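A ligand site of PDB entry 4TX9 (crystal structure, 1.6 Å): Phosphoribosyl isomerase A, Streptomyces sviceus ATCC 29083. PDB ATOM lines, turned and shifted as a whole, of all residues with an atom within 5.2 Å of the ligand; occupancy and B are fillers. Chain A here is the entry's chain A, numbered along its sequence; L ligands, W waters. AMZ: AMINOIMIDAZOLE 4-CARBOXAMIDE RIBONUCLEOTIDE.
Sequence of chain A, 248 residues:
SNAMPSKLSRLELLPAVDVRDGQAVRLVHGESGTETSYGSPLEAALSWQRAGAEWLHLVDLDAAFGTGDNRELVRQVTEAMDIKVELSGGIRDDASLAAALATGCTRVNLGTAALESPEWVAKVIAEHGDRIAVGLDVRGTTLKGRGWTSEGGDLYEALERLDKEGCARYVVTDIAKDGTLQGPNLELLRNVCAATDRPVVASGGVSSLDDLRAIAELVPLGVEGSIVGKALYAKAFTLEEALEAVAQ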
ATOM      1  N   ASP A  18     -15.392 -22.757 -20.912  1.00  0.00           N
ATOM      2  CA  ASP A  18     -14.388 -23.704 -20.391  1.00  0.00           C
ATOM      3  C   ASP A  18     -15.098 -24.535 -19.323  1.00  0.00           C
ATOM      4  O   ASP A  18     -15.671 -23.980 -18.421  1.00  0.00           O
ATOM      5  CB  ASP A  18     -13.180 -22.979 -19.795  1.00  0.00           C
ATOM      6  CG  ASP A  18     -12.529 -22.007 -20.773  1.00  0.00           C
ATOM      7  OD1 ASP A  18     -12.483 -22.281 -21.970  1.00  0.00           O
ATOM      8  OD2 ASP A  18     -12.074 -20.942 -20.319  1.00  0.00           O
ATOM      9  N   LEU A  27     -10.703 -19.304 -14.769  1.00  0.00           N
ATOM     10  CA  LEU A  27      -9.598 -19.444 -13.840  1.00  0.00           C
ATOM     11  C   LEU A  27      -8.721 -18.190 -13.859  1.00  0.00           C
ATOM     12  O   LEU A  27      -9.037 -17.223 -14.562  1.00  0.00           O
ATOM     13  CB  LEU A  27      -8.785 -20.695 -14.180  1.00  0.00           C
ATOM     14  CG  LEU A  27      -9.405 -22.066 -13.881  1.00  0.00           C
ATOM     15  CD1 LEU A  27     -10.695 -22.347 -14.671  1.00  0.00           C
ATOM     16  CD2 LEU A  27      -8.406 -23.134 -14.171  1.00  0.00           C
ATOM     17  N   GLY A  30      -5.001 -19.903 -15.533  1.00  0.00           N
ATOM     18  CA  GLY A  30      -5.342 -21.294 -15.657  1.00  0.00           C
ATOM     19  C   GLY A  30      -4.981 -22.167 -14.475  1.00  0.00           C
ATOM     20  O   GLY A  30      -4.861 -23.371 -14.633  1.00  0.00           O
ATOM     21  N   GLU A  31      -4.848 -21.593 -13.277  1.00  0.00           N
ATOM     22  CA  GLU A  31      -4.381 -22.352 -12.111  1.00  0.00           C
ATOM     23  C   GLU A  31      -5.527 -23.173 -11.522  1.00  0.00           C
ATOM     24  O   GLU A  31      -6.559 -22.619 -11.142  1.00  0.00           O
ATOM     25  CB  GLU A  31      -3.819 -21.437 -11.050  1.00  0.00           C
ATOM     26  CG  GLU A  31      -3.172 -22.156  -9.883  1.00  0.00           C
ATOM     27  CD  GLU A  31      -2.542 -21.183  -8.888  1.00  0.00           C
ATOM     28  OE1 GLU A  31      -2.222 -20.033  -9.280  1.00  0.00           O
ATOM     29  OE2 GLU A  31      -2.365 -21.583  -7.717  1.00  0.00           O
ATOM     30  N   HIS A  57     -15.775 -20.913 -28.472  1.00  0.00           N
ATOM     31  CA  HIS A  57     -14.518 -21.584 -28.129  1.00  0.00           C
ATOM     32  C   HIS A  57     -14.767 -22.467 -26.906  1.00  0.00           C
ATOM     33  O   HIS A  57     -14.888 -21.951 -25.793  1.00  0.00           O
ATOM     34  CB  HIS A  57     -13.389 -20.568 -27.847  1.00  0.00           C
ATOM     35  CG  HIS A  57     -12.074 -21.188 -27.539  1.00  0.00           C
ATOM     36  ND1 HIS A  57     -11.210 -21.633 -28.517  1.00  0.00           N
ATOM     37  CD2 HIS A  57     -11.443 -21.410 -26.355  1.00  0.00           C
ATOM     38  CE1 HIS A  57     -10.102 -22.094 -27.943  1.00  0.00           C
ATOM     39  NE2 HIS A  57     -10.229 -21.982 -26.625  1.00  0.00           N
ATOM     40  N   VAL A  59     -13.893 -25.626 -24.390  1.00  0.00           N
ATOM     41  CA  VAL A  59     -12.743 -26.364 -23.857  1.00  0.00           C
ATOM     42  C   VAL A  59     -13.217 -27.313 -22.754  1.00  0.00           C
ATOM     43  O   VAL A  59     -13.894 -26.889 -21.813  1.00  0.00           O
ATOM     44  CB  VAL A  59     -11.702 -25.412 -23.278  1.00  0.00           C
ATOM     45  CG1 VAL A  59     -10.510 -26.195 -22.801  1.00  0.00           C
ATOM     46  CG2 VAL A  59     -11.272 -24.362 -24.297  1.00  0.00           C
ATOM     47  N   LEU A  61     -11.834 -28.624 -19.879  1.00  0.00           N
ATOM     48  CA  LEU A  61     -10.647 -28.376 -19.027  1.00  0.00           C
ATOM     49  C   LEU A  61     -10.281 -29.588 -18.178  1.00  0.00           C
ATOM     50  O   LEU A  61      -9.086 -29.822 -17.908  1.00  0.00           O
ATOM     51  CB  LEU A  61     -10.882 -27.177 -18.106  1.00  0.00           C
ATOM     52  CG  LEU A  61     -10.633 -25.766 -18.493  1.00  0.00           C
ATOM     53  CD1 LEU A  61     -10.720 -24.961 -17.198  1.00  0.00           C
ATOM     54  CD2 LEU A  61      -9.253 -25.629 -19.116  1.00  0.00           C
ATOM     55  N   ALA A  63     -10.431 -32.555 -19.222  1.00  0.00           N
ATOM     56  CA  ALA A  63      -9.675 -33.395 -20.137  1.00  0.00           C
ATOM     57  C   ALA A  63      -8.263 -32.852 -20.312  1.00  0.00           C
ATOM     58  O   ALA A  63      -7.288 -33.633 -20.463  1.00  0.00           O
ATOM     59  CB  ALA A  63     -10.385 -33.524 -21.459  1.00  0.00           C
ATOM     60  N   ALA A  64      -8.128 -31.537 -20.353  1.00  0.00           N
ATOM     61  CA  ALA A  64      -6.767 -30.930 -20.457  1.00  0.00           C
ATOM     62  C   ALA A  64      -5.924 -31.251 -19.220  1.00  0.00           C
ATOM     63  O   ALA A  64      -4.736 -31.639 -19.334  1.00  0.00           O
ATOM     64  CB  ALA A  64      -6.873 -29.413 -20.674  1.00  0.00           C
ATOM     65  N   PHE A  65      -6.517 -31.154 -18.038  1.00  0.00           N
ATOM     66  CA  PHE A  65      -5.803 -31.445 -16.778  1.00  0.00           C
ATOM     67  C   PHE A  65      -5.595 -32.904 -16.522  1.00  0.00           C
ATOM     68  O   PHE A  65      -4.749 -33.271 -15.693  1.00  0.00           O
ATOM     69  CB  PHE A  65      -6.532 -30.892 -15.569  1.00  0.00           C
ATOM     70  CG  PHE A  65      -6.320 -29.429 -15.326  1.00  0.00           C
ATOM     71  CD1 PHE A  65      -5.097 -28.960 -14.906  1.00  0.00           C
ATOM     72  CD2 PHE A  65      -7.368 -28.548 -15.462  1.00  0.00           C
ATOM     73  CE1 PHE A  65      -4.914 -27.609 -14.659  1.00  0.00           C
ATOM     74  CE2 PHE A  65      -7.185 -27.188 -15.226  1.00  0.00           C
ATOM     75  CZ  PHE A  65      -5.978 -26.734 -14.799  1.00  0.00           C
ATOM     76  N   SER A  88     -11.692 -28.120 -27.914  1.00  0.00           N
ATOM     77  CA  SER A  88     -10.390 -28.579 -27.477  1.00  0.00           C
ATOM     78  C   SER A  88     -10.461 -29.204 -26.097  1.00  0.00           C
ATOM     79  O   SER A  88     -11.492 -29.158 -25.397  1.00  0.00           O
ATOM     80  CB  SER A  88      -9.410 -27.422 -27.490  1.00  0.00           C
ATOM     81  OG  SER A  88      -9.733 -26.456 -26.521  1.00  0.00           O
ATOM     82  N   GLY A  89      -9.329 -29.793 -25.698  1.00  0.00           N
ATOM     83  CA  GLY A  89      -9.173 -30.447 -24.410  1.00  0.00           C
ATOM     84  C   GLY A  89      -9.109 -31.965 -24.562  1.00  0.00           C
ATOM     85  O   GLY A  89     -10.129 -32.640 -24.905  1.00  0.00           O
ATOM     86  N   GLY A  90      -7.933 -32.535 -24.304  1.00  0.00           N
ATOM     87  CA  GLY A  90      -7.718 -33.975 -24.358  1.00  0.00           C
ATOM     88  C   GLY A  90      -7.496 -34.594 -25.723  1.00  0.00           C
ATOM     89  O   GLY A  90      -7.464 -35.832 -25.822  1.00  0.00           O
ATOM     90  N   ILE A  91      -7.349 -33.782 -26.769  1.00  0.00           N
ATOM     91  CA  ILE A  91      -7.304 -34.326 -28.135  1.00  0.00           C
ATOM     92  C   ILE A  91      -5.832 -34.624 -28.431  1.00  0.00           C
ATOM     93  O   ILE A  91      -5.058 -33.756 -28.868  1.00  0.00           O
ATOM     94  CB  ILE A  91      -7.923 -33.405 -29.172  1.00  0.00           C
ATOM     95  CG1 ILE A  91      -9.348 -33.031 -28.791  1.00  0.00           C
ATOM     96  CG2 ILE A  91      -7.873 -34.036 -30.562  1.00  0.00           C
ATOM     97  CD1 ILE A  91      -9.953 -31.955 -29.616  1.00  0.00           C
ATOM     98  N   ARG A  92      -5.453 -35.856 -28.159  1.00  0.00           N
ATOM     99  CA  ARG A  92      -4.042 -36.251 -28.058  1.00  0.00           C
ATOM    100  C   ARG A  92      -3.653 -37.530 -28.782  1.00  0.00           C
ATOM    101  O   ARG A  92      -2.479 -37.919 -28.806  1.00  0.00           O
ATOM    102  CB  ARG A  92      -3.700 -36.410 -26.588  1.00  0.00           C
ATOM    103  CG  ARG A  92      -3.746 -35.092 -25.837  1.00  0.00           C
ATOM    104  CD  ARG A  92      -3.492 -35.266 -24.400  1.00  0.00           C
ATOM    105  NE  ARG A  92      -3.800 -34.041 -23.670  1.00  0.00           N
ATOM    106  CZ  ARG A  92      -3.641 -33.899 -22.357  1.00  0.00           C
ATOM    107  NH1 ARG A  92      -3.128 -34.883 -21.635  1.00  0.00           N
ATOM    108  NH2 ARG A  92      -3.967 -32.760 -21.793  1.00  0.00           N
ATOM    109  N   ASN A 109      -8.679 -27.623 -31.521  1.00  0.00           N
ATOM    110  CA  ASN A 109      -7.331 -27.131 -31.190  1.00  0.00           C
ATOM    111  C   ASN A 109      -6.563 -28.233 -30.488  1.00  0.00           C
ATOM    112  O   ASN A 109      -7.107 -28.900 -29.590  1.00  0.00           O
ATOM    113  CB  ASN A 109      -7.290 -25.919 -30.231  1.00  0.00           C
ATOM    114  CG  ASN A 109      -7.920 -24.670 -30.753  1.00  0.00           C
ATOM    115  OD1 ASN A 109      -8.043 -23.684 -29.980  1.00  0.00           O
ATOM    116  ND2 ASN A 109      -8.266 -24.629 -32.036  1.00  0.00           N
ATOM    117  N   LEU A 110      -5.306 -28.426 -30.894  1.00  0.00           N
ATOM    118  CA  LEU A 110      -4.406 -29.373 -30.222  1.00  0.00           C
ATOM    119  C   LEU A 110      -3.406 -28.598 -29.400  1.00  0.00           C
ATOM    120  O   LEU A 110      -2.743 -27.723 -29.942  1.00  0.00           O
ATOM    121  CB  LEU A 110      -3.671 -30.231 -31.240  1.00  0.00           C
ATOM    122  CG  LEU A 110      -4.542 -30.803 -32.351  1.00  0.00           C
ATOM    123  CD1 LEU A 110      -3.642 -31.502 -33.381  1.00  0.00           C
ATOM    124  CD2 LEU A 110      -5.556 -31.733 -31.750  1.00  0.00           C
ATOM    125  N   GLY A 111      -3.204 -28.985 -28.139  1.00  0.00           N
ATOM    126  CA  GLY A 111      -2.220 -28.329 -27.275  1.00  0.00           C
ATOM    127  C   GLY A 111      -1.061 -29.247 -26.930  1.00  0.00           C
ATOM    128  O   GLY A 111      -0.017 -29.210 -27.575  1.00  0.00           O
ATOM    129  N   THR A 112      -1.260 -30.091 -25.907  1.00  0.00           N
ATOM    130  CA  THR A 112      -0.231 -31.007 -25.435  1.00  0.00           C
ATOM    131  C   THR A 112       0.379 -31.811 -26.546  1.00  0.00           C
ATOM    132  O   THR A 112       1.577 -32.090 -26.520  1.00  0.00           O
ATOM    133  CB  THR A 112      -0.827 -31.971 -24.353  1.00  0.00           C
ATOM    134  OG1 THR A 112      -1.288 -31.176 -23.249  1.00  0.00           O
ATOM    135  CG2 THR A 112       0.189 -32.956 -23.855  1.00  0.00           C
ATOM    136  N   ALA A 113      -0.443 -32.302 -27.479  1.00  0.00           N
ATOM    137  CA  ALA A 113       0.092 -33.193 -28.502  1.00  0.00           C
ATOM    138  C   ALA A 113       1.132 -32.524 -29.376  1.00  0.00           C
ATOM    139  O   ALA A 113       2.029 -33.186 -29.869  1.00  0.00           O
ATOM    140  CB  ALA A 113      -1.016 -33.727 -29.379  1.00  0.00           C
ATOM    141  N   ASP A 137       0.218 -22.118 -25.937  1.00  0.00           N
ATOM    142  CA  ASP A 137      -0.041 -21.423 -24.673  1.00  0.00           C
ATOM    143  C   ASP A 137       1.256 -21.269 -23.956  1.00  0.00           C
ATOM    144  O   ASP A 137       1.943 -22.240 -23.696  1.00  0.00           O
ATOM    145  CB  ASP A 137      -1.054 -22.226 -23.870  1.00  0.00           C
ATOM    146  CG  ASP A 137      -2.377 -22.352 -24.598  1.00  0.00           C
ATOM    147  OD1 ASP A 137      -2.726 -21.493 -25.449  1.00  0.00           O
ATOM    148  OD2 ASP A 137      -3.097 -23.325 -24.312  1.00  0.00           O
ATOM    149  N   ARG A 146      -0.514 -30.073 -20.770  1.00  0.00           N
ATOM    150  CA  ARG A 146      -1.197 -30.756 -19.703  1.00  0.00           C
ATOM    151  C   ARG A 146      -1.926 -29.806 -18.721  1.00  0.00           C
ATOM    152  O   ARG A 146      -1.758 -29.902 -17.506  1.00  0.00           O
ATOM    153  CB  ARG A 146      -0.225 -31.657 -18.981  1.00  0.00           C
ATOM    154  CG  ARG A 146       0.236 -32.780 -19.912  1.00  0.00           C
ATOM    155  CD  ARG A 146       0.885 -33.918 -19.239  1.00  0.00           C
ATOM    156  NE  ARG A 146       1.138 -34.982 -20.208  1.00  0.00           N
ATOM    157  CZ  ARG A 146       0.469 -36.126 -20.287  1.00  0.00           C
ATOM    158  NH1 ARG A 146      -0.511 -36.431 -19.435  1.00  0.00           N
ATOM    159  NH2 ARG A 146       0.817 -37.010 -21.219  1.00  0.00           N
ATOM    160  N   GLY A 147      -2.737 -28.930 -19.284  1.00  0.00           N
ATOM    161  CA  GLY A 147      -3.507 -28.011 -18.432  1.00  0.00           C
ATOM    162  C   GLY A 147      -2.614 -26.896 -17.912  1.00  0.00           C
ATOM    163  O   GLY A 147      -2.944 -26.218 -16.919  1.00  0.00           O
ATOM    164  N   TRP A 148      -1.486 -26.738 -18.592  1.00  0.00           N
ATOM    165  CA  TRP A 148      -0.429 -25.750 -18.365  1.00  0.00           C
ATOM    166  C   TRP A 148       0.453 -26.120 -17.161  1.00  0.00           C
ATOM    167  O   TRP A 148       1.116 -25.252 -16.560  1.00  0.00           O
ATOM    168  CB  TRP A 148      -1.007 -24.345 -18.206  1.00  0.00           C
ATOM    169  CG  TRP A 148      -1.812 -23.890 -19.411  1.00  0.00           C
ATOM    170  CD1 TRP A 148      -1.828 -24.451 -20.651  1.00  0.00           C
ATOM    171  CD2 TRP A 148      -2.717 -22.793 -19.476  1.00  0.00           C
ATOM    172  NE1 TRP A 148      -2.662 -23.772 -21.486  1.00  0.00           N
ATOM    173  CE2 TRP A 148      -3.239 -22.743 -20.776  1.00  0.00           C
ATOM    174  CE3 TRP A 148      -3.113 -21.819 -18.559  1.00  0.00           C
ATOM    175  CZ2 TRP A 148      -4.135 -21.773 -21.196  1.00  0.00           C
ATOM    176  CZ3 TRP A 148      -4.030 -20.851 -18.969  1.00  0.00           C
ATOM    177  CH2 TRP A 148      -4.552 -20.854 -20.267  1.00  0.00           C
ATOM    178  N   THR A 173      -2.258 -18.241 -26.433  1.00  0.00           N
ATOM    179  CA  THR A 173      -2.668 -17.713 -25.119  1.00  0.00           C
ATOM    180  C   THR A 173      -1.466 -17.241 -24.361  1.00  0.00           C
ATOM    181  O   THR A 173      -0.497 -17.991 -24.233  1.00  0.00           O
ATOM    182  CB  THR A 173      -3.375 -18.765 -24.235  1.00  0.00           C
ATOM    183  OG1 THR A 173      -4.466 -19.374 -24.955  1.00  0.00           O
ATOM    184  CG2 THR A 173      -3.899 -18.133 -22.949  1.00  0.00           C
ATOM    185  N   ASP A 178      -4.194 -14.625 -18.744  1.00  0.00           N
ATOM    186  CA  ASP A 178      -5.450 -15.286 -18.790  1.00  0.00           C
ATOM    187  C   ASP A 178      -6.180 -15.225 -17.447  1.00  0.00           C
ATOM    188  O   ASP A 178      -5.611 -15.524 -16.392  1.00  0.00           O
ATOM    189  CB  ASP A 178      -5.254 -16.711 -19.256  1.00  0.00           C
ATOM    190  CG  ASP A 178      -6.491 -17.291 -19.880  1.00  0.00           C
ATOM    191  OD1 ASP A 178      -7.103 -18.133 -19.198  1.00  0.00           O
ATOM    192  OD2 ASP A 178      -6.876 -16.879 -21.010  1.00  0.00           O
HETATM  193  O5  AMZ L   1      -6.965 -22.968 -18.155  1.00  0.00           O
HETATM  194  C6  AMZ L   1      -6.202 -23.917 -18.316  1.00  0.00           C
HETATM  195  N2  AMZ L   1      -5.379 -24.440 -17.411  1.00  0.00           N
HETATM  196  C3A AMZ L   1      -6.046 -24.561 -19.624  1.00  0.00           C
HETATM  197  C7A AMZ L   1      -6.689 -24.301 -20.786  1.00  0.00           C
HETATM  198  N3  AMZ L   1      -7.597 -23.286 -21.060  1.00  0.00           N
HETATM  199  N1  AMZ L   1      -5.230 -25.635 -19.842  1.00  0.00           N
HETATM  200  C5  AMZ L   1      -5.389 -25.997 -21.105  1.00  0.00           C
HETATM  201  N   AMZ L   1      -6.273 -25.147 -21.692  1.00  0.00           N
HETATM  202  C1  AMZ L   1      -6.743 -25.286 -23.083  1.00  0.00           C
HETATM  203  C2  AMZ L   1      -5.782 -24.891 -24.161  1.00  0.00           C
HETATM  204  C3  AMZ L   1      -6.358 -25.684 -25.322  1.00  0.00           C
HETATM  205  O2  AMZ L   1      -7.531 -24.990 -25.825  1.00  0.00           O
HETATM  206  O1  AMZ L   1      -5.830 -23.475 -24.299  1.00  0.00           O
HETATM  207  O   AMZ L   1      -6.952 -26.710 -23.260  1.00  0.00           O
HETATM  208  C   AMZ L   1      -6.711 -27.005 -24.649  1.00  0.00           C
HETATM  209  C4  AMZ L   1      -5.564 -27.960 -24.885  1.00  0.00           C
HETATM  210  O3  AMZ L   1      -5.855 -29.256 -24.331  1.00  0.00           O
HETATM  211  P   AMZ L   1      -4.840 -30.429 -24.659  1.00  0.00           P
HETATM  212  OP1 AMZ L   1      -3.472 -29.990 -24.083  1.00  0.00           O
HETATM  213  O4  AMZ L   1      -4.780 -30.520 -26.163  1.00  0.00           O
HETATM  214  OP2 AMZ L   1      -5.431 -31.587 -23.895  1.00  0.00           O
HETATM  215  O   HOH W   1      -3.149 -28.279 -22.013  1.00  0.00           O
HETATM  216  O   HOH W   2      -8.294 -22.101 -24.595  1.00  0.00           O
HETATM  217  O   HOH W   3      -3.251 -32.152 -27.594  1.00  0.00           O
HETATM  218  O   HOH W   4      -7.966 -20.589 -17.819  1.00  0.00           O
HETATM  219  O   HOH W   5      -6.826 -23.164 -27.622  1.00  0.00           O
HETATM  220  O   HOH W   6      -7.168 -30.599 -27.264  1.00  0.00           O
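OD1 of Asp 137 lies within hydrogen-bond range of OG1 of Thr 173 (2.8 Å). NH2 of Arg 92 is in hydrogen-bond range of OG1 of Thr 112 (3.4 Å). OD2 of Asp 137 lies within hydrogen-bond range of NE1 of Trp 148 (2.9 Å). The backbone carbonyl oxygen (O) of Ala 64 is in hydrogen-bond range of the backbone NH (N) of Gly 147 (3.4 Å). OG1 of Thr 112 is in hydrogen-bond range of N of Arg 146 (2.8 Å). NH2 of Arg 92 lies within hydrogen-bond range of O of Ala 64, 2.8 Å away.
Merely in contact with the ligand: Val 59, Leu 61, Ala 64, Phe 65, Gly 89 and Trp 148. Hydrophobic or aromatic side chains within 4 Å of the ligand: Val 59, Leu 61, Ala 64, Phe 65 and Trp 148. Of the 26 residues printed, 14 come within 4 Å of the ligand.
Water W4 bridges O5 of the ligand (2.6 Å) and OD1 of Asp 178 (2.9 Å). Water W6 lies within hydrogen-bond range of O4 of the ligand (2.6 Å), N of Gly 89 (2.8 Å), O of Asn 109 (2.9 Å) and N of Ile 91 (3.2 Å). Water W5 bridges O2 of the ligand (2.7 Å) and OD1 of Asn 109 (2.7 Å). Water W1 lies within hydrogen-bond range of OP1 of the ligand (2.7 Å), N of Gly 147 (2.8 Å) and N of Arg 146 (3.4 Å). Water W2 bridges NE2 of His 57 and O1 of the ligand.
OG of Ser 88 lies within hydrogen-bond range of O2 of the ligand (2.7 Å). OP1 of the ligand is in hydrogen-bond range of N of Thr 112 (2.9 Å). NH2 of Arg 92 lies within salt-bridge range of OP2 of the ligand. An oxygen (O1) of the ligand is in hydrogen-bond range of the side-chain carboxylate (OD2) of Asp 137 (2.7 Å). An oxygen (OP1) of the ligand sits at hydrogen-bond distance from the side-chain hydroxyl (OG1) of Thr 112 (2.6 Å). O4 of the ligand lies within hydrogen-bond range of N of Gly 111. O of Gly 147 is in hydrogen-bond range of N2 of the ligand, at 3.1 Å. The backbone carbonyl oxygen (O) of Gly 30 sits at hydrogen-bond distance from a nitrogen (N2) of the ligand (3.0 Å). N of Gly 90 sits at hydrogen-bond distance from OP2 of the ligand (2.7 Å).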
